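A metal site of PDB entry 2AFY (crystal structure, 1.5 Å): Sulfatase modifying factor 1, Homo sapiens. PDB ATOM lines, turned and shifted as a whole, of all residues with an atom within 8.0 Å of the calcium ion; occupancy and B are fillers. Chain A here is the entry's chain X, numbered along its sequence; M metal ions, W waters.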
ATOM      1  N   TYR A  44      17.443   6.059  -9.258  1.00  0.00           N
ATOM      2  CA  TYR A  44      17.281   5.811  -7.839  1.00  0.00           C
ATOM      3  C   TYR A  44      15.818   5.588  -7.468  1.00  0.00           C
ATOM      4  O   TYR A  44      14.922   6.127  -8.105  1.00  0.00           O
ATOM      5  CB  TYR A  44      17.711   7.059  -7.043  1.00  0.00           C
ATOM      6  CG  TYR A  44      19.067   7.565  -7.417  1.00  0.00           C
ATOM      7  CD1 TYR A  44      20.195   6.874  -7.080  1.00  0.00           C
ATOM      8  CD2 TYR A  44      19.236   8.766  -8.118  1.00  0.00           C
ATOM      9  CE1 TYR A  44      21.464   7.315  -7.428  1.00  0.00           C
ATOM     10  CE2 TYR A  44      20.506   9.215  -8.435  1.00  0.00           C
ATOM     11  CZ  TYR A  44      21.618   8.486  -8.091  1.00  0.00           C
ATOM     12  OH  TYR A  44      22.905   8.909  -8.396  1.00  0.00           O
ATOM     13  N   GLU A  45      15.568   4.773  -6.441  1.00  0.00           N
ATOM     14  CA  GLU A  45      14.258   4.817  -5.812  1.00  0.00           C
ATOM     15  C   GLU A  45      13.928   6.266  -5.443  1.00  0.00           C
ATOM     16  O   GLU A  45      14.827   7.035  -5.126  1.00  0.00           O
ATOM     17  CB  GLU A  45      14.272   3.986  -4.543  1.00  0.00           C
ATOM     18  CG  GLU A  45      14.579   2.514  -4.784  1.00  0.00           C
ATOM     19  CD  GLU A  45      15.240   1.792  -3.597  1.00  0.00           C
ATOM     20  OE1 GLU A  45      16.053   2.416  -2.890  1.00  0.00           O
ATOM     21  OE2 GLU A  45      14.949   0.576  -3.401  1.00  0.00           O
ATOM     22  N   PRO A 120      14.873   5.758   0.614  1.00  0.00           N
ATOM     23  CA  PRO A 120      13.668   5.640  -0.188  1.00  0.00           C
ATOM     24  C   PRO A 120      12.434   5.965   0.618  1.00  0.00           C
ATOM     25  O   PRO A 120      12.319   5.592   1.781  1.00  0.00           O
ATOM     26  CB  PRO A 120      13.672   4.155  -0.617  1.00  0.00           C
ATOM     27  CG  PRO A 120      14.455   3.474   0.437  1.00  0.00           C
ATOM     28  CD  PRO A 120      15.552   4.457   0.786  1.00  0.00           C
ATOM     29  N   TRP A 146      10.616  -2.811 -16.095  1.00  0.00           N
ATOM     30  CA  TRP A 146      11.316  -2.885 -14.815  1.00  0.00           C
ATOM     31  C   TRP A 146      12.313  -4.042 -14.846  1.00  0.00           C
ATOM     32  O   TRP A 146      13.507  -3.904 -14.460  1.00  0.00           O
ATOM     33  CB  TRP A 146      10.307  -3.003 -13.645  1.00  0.00           C
ATOM     34  CG  TRP A 146      10.957  -2.877 -12.310  1.00  0.00           C
ATOM     35  CD1 TRP A 146      10.961  -1.773 -11.510  1.00  0.00           C
ATOM     36  CD2 TRP A 146      11.745  -3.858 -11.653  1.00  0.00           C
ATOM     37  NE1 TRP A 146      11.684  -2.018 -10.370  1.00  0.00           N
ATOM     38  CE2 TRP A 146      12.162  -3.301 -10.421  1.00  0.00           C
ATOM     39  CE3 TRP A 146      12.084  -5.190 -11.928  1.00  0.00           C
ATOM     40  CZ2 TRP A 146      12.986  -3.978  -9.543  1.00  0.00           C
ATOM     41  CZ3 TRP A 146      12.890  -5.855 -11.043  1.00  0.00           C
ATOM     42  CH2 TRP A 146      13.328  -5.244  -9.867  1.00  0.00           C
ATOM     43  N   ASN A 174      21.077  -4.263  -0.560  1.00  0.00           N
ATOM     44  CA  ASN A 174      20.653  -4.227   0.832  1.00  0.00           C
ATOM     45  C   ASN A 174      19.495  -5.218   1.030  1.00  0.00           C
ATOM     46  O   ASN A 174      18.351  -4.923   0.726  1.00  0.00           O
ATOM     47  CB  ASN A 174      20.202  -2.827   1.192  1.00  0.00           C
ATOM     48  CG  ASN A 174      19.756  -2.694   2.612  1.00  0.00           C
ATOM     49  OD1 ASN A 174      20.074  -3.551   3.441  1.00  0.00           O
ATOM     50  ND2 ASN A 174      18.986  -1.629   2.920  1.00  0.00           N
ATOM     51  N   TYR A 207      20.554   2.006  -9.288  1.00  0.00           N
ATOM     52  CA  TYR A 207      20.916   1.703  -7.911  1.00  0.00           C
ATOM     53  C   TYR A 207      19.746   1.041  -7.206  1.00  0.00           C
ATOM     54  O   TYR A 207      18.607   1.475  -7.366  1.00  0.00           O
ATOM     55  CB  TYR A 207      21.276   3.010  -7.196  1.00  0.00           C
ATOM     56  CG  TYR A 207      22.521   3.660  -7.717  1.00  0.00           C
ATOM     57  CD1 TYR A 207      22.497   4.390  -8.897  1.00  0.00           C
ATOM     58  CD2 TYR A 207      23.742   3.492  -7.067  1.00  0.00           C
ATOM     59  CE1 TYR A 207      23.648   4.944  -9.404  1.00  0.00           C
ATOM     60  CE2 TYR A 207      24.908   4.071  -7.561  1.00  0.00           C
ATOM     61  CZ  TYR A 207      24.854   4.796  -8.725  1.00  0.00           C
ATOM     62  OH  TYR A 207      26.008   5.372  -9.231  1.00  0.00           O
ATOM     63  N   ASN A 208      20.058   0.009  -6.420  1.00  0.00           N
ATOM     64  CA  ASN A 208      19.103  -0.620  -5.500  1.00  0.00           C
ATOM     65  C   ASN A 208      17.866  -1.108  -6.199  1.00  0.00           C
ATOM     66  O   ASN A 208      16.801  -1.144  -5.614  1.00  0.00           O
ATOM     67  CB  ASN A 208      18.770   0.325  -4.357  1.00  0.00           C
ATOM     68  CG  ASN A 208      19.999   0.648  -3.560  1.00  0.00           C
ATOM     69  OD1 ASN A 208      20.609  -0.264  -2.959  1.00  0.00           O
ATOM     70  ND2 ASN A 208      20.426   1.912  -3.613  1.00  0.00           N
ATOM     71  N   ILE A 209      18.038  -1.537  -7.442  1.00  0.00           N
ATOM     72  CA  ILE A 209      16.903  -2.116  -8.187  1.00  0.00           C
ATOM     73  C   ILE A 209      16.486  -3.484  -7.617  1.00  0.00           C
ATOM     74  O   ILE A 209      15.296  -3.817  -7.620  1.00  0.00           O
ATOM     75  CB  ILE A 209      17.172  -2.088  -9.724  1.00  0.00           C
ATOM     76  CG1 ILE A 209      15.892  -2.377 -10.509  1.00  0.00           C
ATOM     77  CG2 ILE A 209      18.264  -3.026 -10.103  1.00  0.00           C
ATOM     78  CD1 ILE A 209      15.029  -1.201 -10.711  1.00  0.00           C
ATOM     79  N   VAL A 210      17.432  -4.268  -7.076  1.00  0.00           N
ATOM     80  CA  VAL A 210      17.054  -5.314  -6.132  1.00  0.00           C
ATOM     81  C   VAL A 210      17.433  -4.861  -4.724  1.00  0.00           C
ATOM     82  O   VAL A 210      18.435  -4.162  -4.524  1.00  0.00           O
ATOM     83  CB  VAL A 210      17.618  -6.715  -6.424  1.00  0.00           C
ATOM     84  CG1 VAL A 210      17.149  -7.211  -7.765  1.00  0.00           C
ATOM     85  CG2 VAL A 210      19.122  -6.786  -6.306  1.00  0.00           C
ATOM     86  N   GLY A 211      16.611  -5.258  -3.751  1.00  0.00           N
ATOM     87  CA  GLY A 211      16.838  -4.853  -2.387  1.00  0.00           C
ATOM     88  C   GLY A 211      16.447  -3.429  -2.069  1.00  0.00           C
ATOM     89  O   GLY A 211      15.954  -2.681  -2.915  1.00  0.00           O
ATOM     90  N   ASN A 212      16.633  -3.082  -0.792  1.00  0.00           N
ATOM     91  CA  ASN A 212      16.345  -1.759  -0.227  1.00  0.00           C
ATOM     92  C   ASN A 212      14.835  -1.642  -0.082  1.00  0.00           C
ATOM     93  O   ASN A 212      14.301  -2.271   0.842  1.00  0.00           O
ATOM     94  CB  ASN A 212      17.018  -0.587  -0.972  1.00  0.00           C
ATOM     95  CG  ASN A 212      17.462   0.523  -0.013  1.00  0.00           C
ATOM     96  OD1 ASN A 212      17.755   0.255   1.162  1.00  0.00           O
ATOM     97  ND2 ASN A 212      17.532   1.768  -0.506  1.00  0.00           N
ATOM     98  N   ALA A 213      14.138  -0.943  -0.960  1.00  0.00           N
ATOM     99  CA  ALA A 213      12.661  -0.952  -0.974  1.00  0.00           C
ATOM    100  C   ALA A 213      12.175  -1.801  -2.139  1.00  0.00           C
ATOM    101  O   ALA A 213      12.755  -1.748  -3.223  1.00  0.00           O
ATOM    102  CB  ALA A 213      12.113   0.451  -1.114  1.00  0.00           C
ATOM    103  N   TRP A 214      11.109  -2.561  -1.945  1.00  0.00           N
ATOM    104  CA  TRP A 214      10.344  -3.112  -3.048  1.00  0.00           C
ATOM    105  C   TRP A 214       9.893  -1.991  -3.976  1.00  0.00           C
ATOM    106  O   TRP A 214       9.760  -0.837  -3.520  1.00  0.00           O
ATOM    107  CB  TRP A 214       9.067  -3.810  -2.552  1.00  0.00           C
ATOM    108  CG  TRP A 214       9.201  -5.221  -2.070  1.00  0.00           C
ATOM    109  CD1 TRP A 214       9.335  -5.636  -0.779  1.00  0.00           C
ATOM    110  CD2 TRP A 214       9.092  -6.401  -2.857  1.00  0.00           C
ATOM    111  NE1 TRP A 214       9.363  -7.023  -0.718  1.00  0.00           N
ATOM    112  CE2 TRP A 214       9.231  -7.518  -1.987  1.00  0.00           C
ATOM    113  CE3 TRP A 214       8.933  -6.622  -4.209  1.00  0.00           C
ATOM    114  CZ2 TRP A 214       9.159  -8.822  -2.446  1.00  0.00           C
ATOM    115  CZ3 TRP A 214       8.902  -7.955  -4.672  1.00  0.00           C
ATOM    116  CH2 TRP A 214       9.008  -9.013  -3.796  1.00  0.00           C
ATOM    117  N   GLU A 215       9.563  -2.326  -5.224  1.00  0.00           N
ATOM    118  CA  GLU A 215       9.169  -1.290  -6.184  1.00  0.00           C
ATOM    119  C   GLU A 215       7.890  -1.607  -6.949  1.00  0.00           C
ATOM    120  O   GLU A 215       7.773  -2.614  -7.594  1.00  0.00           O
ATOM    121  CB  GLU A 215      10.346  -1.032  -7.135  1.00  0.00           C
ATOM    122  CG  GLU A 215      11.574  -0.709  -6.337  1.00  0.00           C
ATOM    123  CD  GLU A 215      12.825  -0.422  -7.145  1.00  0.00           C
ATOM    124  OE1 GLU A 215      12.757  -0.245  -8.357  1.00  0.00           O
ATOM    125  OE2 GLU A 215      13.929  -0.381  -6.531  1.00  0.00           O
ATOM    126  N   LYS A 245       8.186  -5.499  -7.590  1.00  0.00           N
ATOM    127  CA  LYS A 245       9.422  -6.183  -7.964  1.00  0.00           C
ATOM    128  C   LYS A 245      10.618  -5.821  -7.090  1.00  0.00           C
ATOM    129  O   LYS A 245      10.651  -4.765  -6.468  1.00  0.00           O
ATOM    130  CB  LYS A 245       9.777  -5.823  -9.394  1.00  0.00           C
ATOM    131  CG  LYS A 245       8.736  -6.212 -10.447  1.00  0.00           C
ATOM    132  CD  LYS A 245       8.804  -7.698 -10.815  1.00  0.00           C
ATOM    133  CE  LYS A 245       9.861  -8.016 -11.891  1.00  0.00           C
ATOM    134  NZ  LYS A 245       9.760  -9.497 -12.346  1.00  0.00           N
ATOM    135  N   GLY A 246      11.574  -6.733  -7.085  1.00  0.00           N
ATOM    136  CA  GLY A 246      12.924  -6.438  -6.663  1.00  0.00           C
ATOM    137  C   GLY A 246      13.336  -6.768  -5.248  1.00  0.00           C
ATOM    138  O   GLY A 246      14.544  -6.786  -4.962  1.00  0.00           O
ATOM    139  N   GLY A 247      12.393  -7.058  -4.363  1.00  0.00           N
ATOM    140  CA  GLY A 247      12.745  -7.328  -2.997  1.00  0.00           C
ATOM    141  C   GLY A 247      13.238  -6.105  -2.252  1.00  0.00           C
ATOM    142  O   GLY A 247      13.279  -4.994  -2.781  1.00  0.00           O
ATOM    143  N   SER A 248      13.592  -6.339  -0.996  1.00  0.00           N
ATOM    144  CA  SER A 248      13.828  -5.293  -0.029  1.00  0.00           C
ATOM    145  C   SER A 248      14.880  -5.692   0.988  1.00  0.00           C
ATOM    146  O   SER A 248      15.403  -6.816   0.976  1.00  0.00           O
ATOM    147  CB  SER A 248      12.538  -4.971   0.718  1.00  0.00           C
ATOM    148  OG  SER A 248      12.222  -5.978   1.692  1.00  0.00           O
ATOM    149  N   TYR A 249      15.129  -4.774   1.915  1.00  0.00           N
ATOM    150  CA  TYR A 249      16.062  -4.991   3.027  1.00  0.00           C
ATOM    151  C   TYR A 249      15.693  -6.137   3.930  1.00  0.00           C
ATOM    152  O   TYR A 249      16.499  -6.552   4.767  1.00  0.00           O
ATOM    153  CB  TYR A 249      16.226  -3.694   3.843  1.00  0.00           C
ATOM    154  CG  TYR A 249      15.011  -3.243   4.623  1.00  0.00           C
ATOM    155  CD1 TYR A 249      14.154  -2.257   4.128  1.00  0.00           C
ATOM    156  CD2 TYR A 249      14.755  -3.762   5.874  1.00  0.00           C
ATOM    157  CE1 TYR A 249      13.062  -1.829   4.886  1.00  0.00           C
ATOM    158  CE2 TYR A 249      13.649  -3.358   6.610  1.00  0.00           C
ATOM    159  CZ  TYR A 249      12.817  -2.389   6.118  1.00  0.00           C
ATOM    160  OH  TYR A 249      11.744  -1.986   6.878  1.00  0.00           O
ATOM    161  N   ASN A 275       8.472  -1.520   3.753  1.00  0.00           N
ATOM    162  CA  ASN A 275       9.539  -2.005   2.889  1.00  0.00           C
ATOM    163  C   ASN A 275       9.194  -1.837   1.412  1.00  0.00           C
ATOM    164  O   ASN A 275       9.798  -2.493   0.587  1.00  0.00           O
ATOM    165  CB  ASN A 275       9.855  -3.482   3.166  1.00  0.00           C
ATOM    166  CG  ASN A 275       8.743  -4.396   2.744  1.00  0.00           C
ATOM    167  OD1 ASN A 275       7.631  -3.959   2.497  1.00  0.00           O
ATOM    168  ND2 ASN A 275       9.040  -5.724   2.685  1.00  0.00           N
ATOM    169  N   GLY A 277       8.414   0.869  -1.797  1.00  0.00           N
ATOM    170  CA  GLY A 277       8.531   2.185  -2.433  1.00  0.00           C
ATOM    171  C   GLY A 277       8.377   2.026  -3.936  1.00  0.00           C
ATOM    172  O   GLY A 277       7.591   1.209  -4.418  1.00  0.00           O
ATOM    173  N   PHE A 278       9.118   2.822  -4.695  1.00  0.00           N
ATOM    174  CA  PHE A 278       8.987   2.848  -6.131  1.00  0.00           C
ATOM    175  C   PHE A 278      10.048   3.751  -6.779  1.00  0.00           C
ATOM    176  O   PHE A 278      10.690   4.560  -6.106  1.00  0.00           O
ATOM    177  CB  PHE A 278       7.597   3.342  -6.571  1.00  0.00           C
ATOM    178  CG  PHE A 278       7.328   4.793  -6.274  1.00  0.00           C
ATOM    179  CD1 PHE A 278       7.343   5.734  -7.284  1.00  0.00           C
ATOM    180  CD2 PHE A 278       7.023   5.200  -4.991  1.00  0.00           C
ATOM    181  CE1 PHE A 278       7.097   7.060  -6.995  1.00  0.00           C
ATOM    182  CE2 PHE A 278       6.760   6.529  -4.735  1.00  0.00           C
ATOM    183  CZ  PHE A 278       6.832   7.451  -5.716  1.00  0.00           C
ATOM    184  N   ARG A 279      10.174   3.572  -8.097  1.00  0.00           N
ATOM    185  CA  ARG A 279      10.888   4.534  -8.960  1.00  0.00           C
ATOM    186  C   ARG A 279      10.017   4.795 -10.193  1.00  0.00           C
ATOM    187  O   ARG A 279       9.122   4.012 -10.519  1.00  0.00           O
ATOM    188  CB  ARG A 279      12.266   4.024  -9.361  1.00  0.00           C
ATOM    189  CG  ARG A 279      12.277   2.976 -10.422  1.00  0.00           C
ATOM    190  CD  ARG A 279      13.708   2.462 -10.694  1.00  0.00           C
ATOM    191  NE  ARG A 279      14.282   1.769  -9.541  1.00  0.00           N
ATOM    192  CZ  ARG A 279      15.533   1.883  -9.075  1.00  0.00           C
ATOM    193  NH1 ARG A 279      16.410   2.698  -9.652  1.00  0.00           N
ATOM    194  NH2 ARG A 279      15.880   1.185  -7.997  1.00  0.00           N
HETATM  195 CA    CA M   1      14.721  -1.397  -4.548  1.00  0.00          CA
HETATM  196  O   HOH W   1      13.912  -3.506  -5.259  1.00  0.00           O
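The calcium ion is bound by the side-chain carboxylate of Glu 45, the backbone carbonyl oxygen of Asn 208, the side-chain carboxylate of Glu 215, water W1, the backbone carbonyl oxygen of Ala 213 and the backbone carbonyl oxygen of Gly 211.
The guanidinium group of Arg 279 lies close to the backbone carbonyl oxygen of Asn 208, at 3.5 Å. The backbone carbonyl oxygen of Glu 215 sits at hydrogen-bond distance from the backbone NH of Lys 245 (2.9 Å). The indole nitrogen (NE1) of Trp 146 lies within hydrogen-bond range of the side-chain carboxylate (OE1) of Glu 215 (2.9 Å). The backbone carbonyl oxygen (O) of Gly 246 lies within hydrogen-bond range of the backbone NH (N) of Gly 211. N of Gly 211 sits at hydrogen-bond distance from O of Gly 247, at 3.5 Å. The side-chain carboxylate (OE1) of Glu 45 lies within hydrogen-bond range of the side-chain amide nitrogen (ND2) of Asn 212, 2.9 Å away. The guanidinium group (NE) of Arg 279 lies within salt-bridge range of the side-chain carboxylate (OE1) of Glu 215, at 2.8 Å.
Residues that only touch the calcium ion: Ile 209. Of the 23 residues printed, 6 come within 4 Å of the calcium ion.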
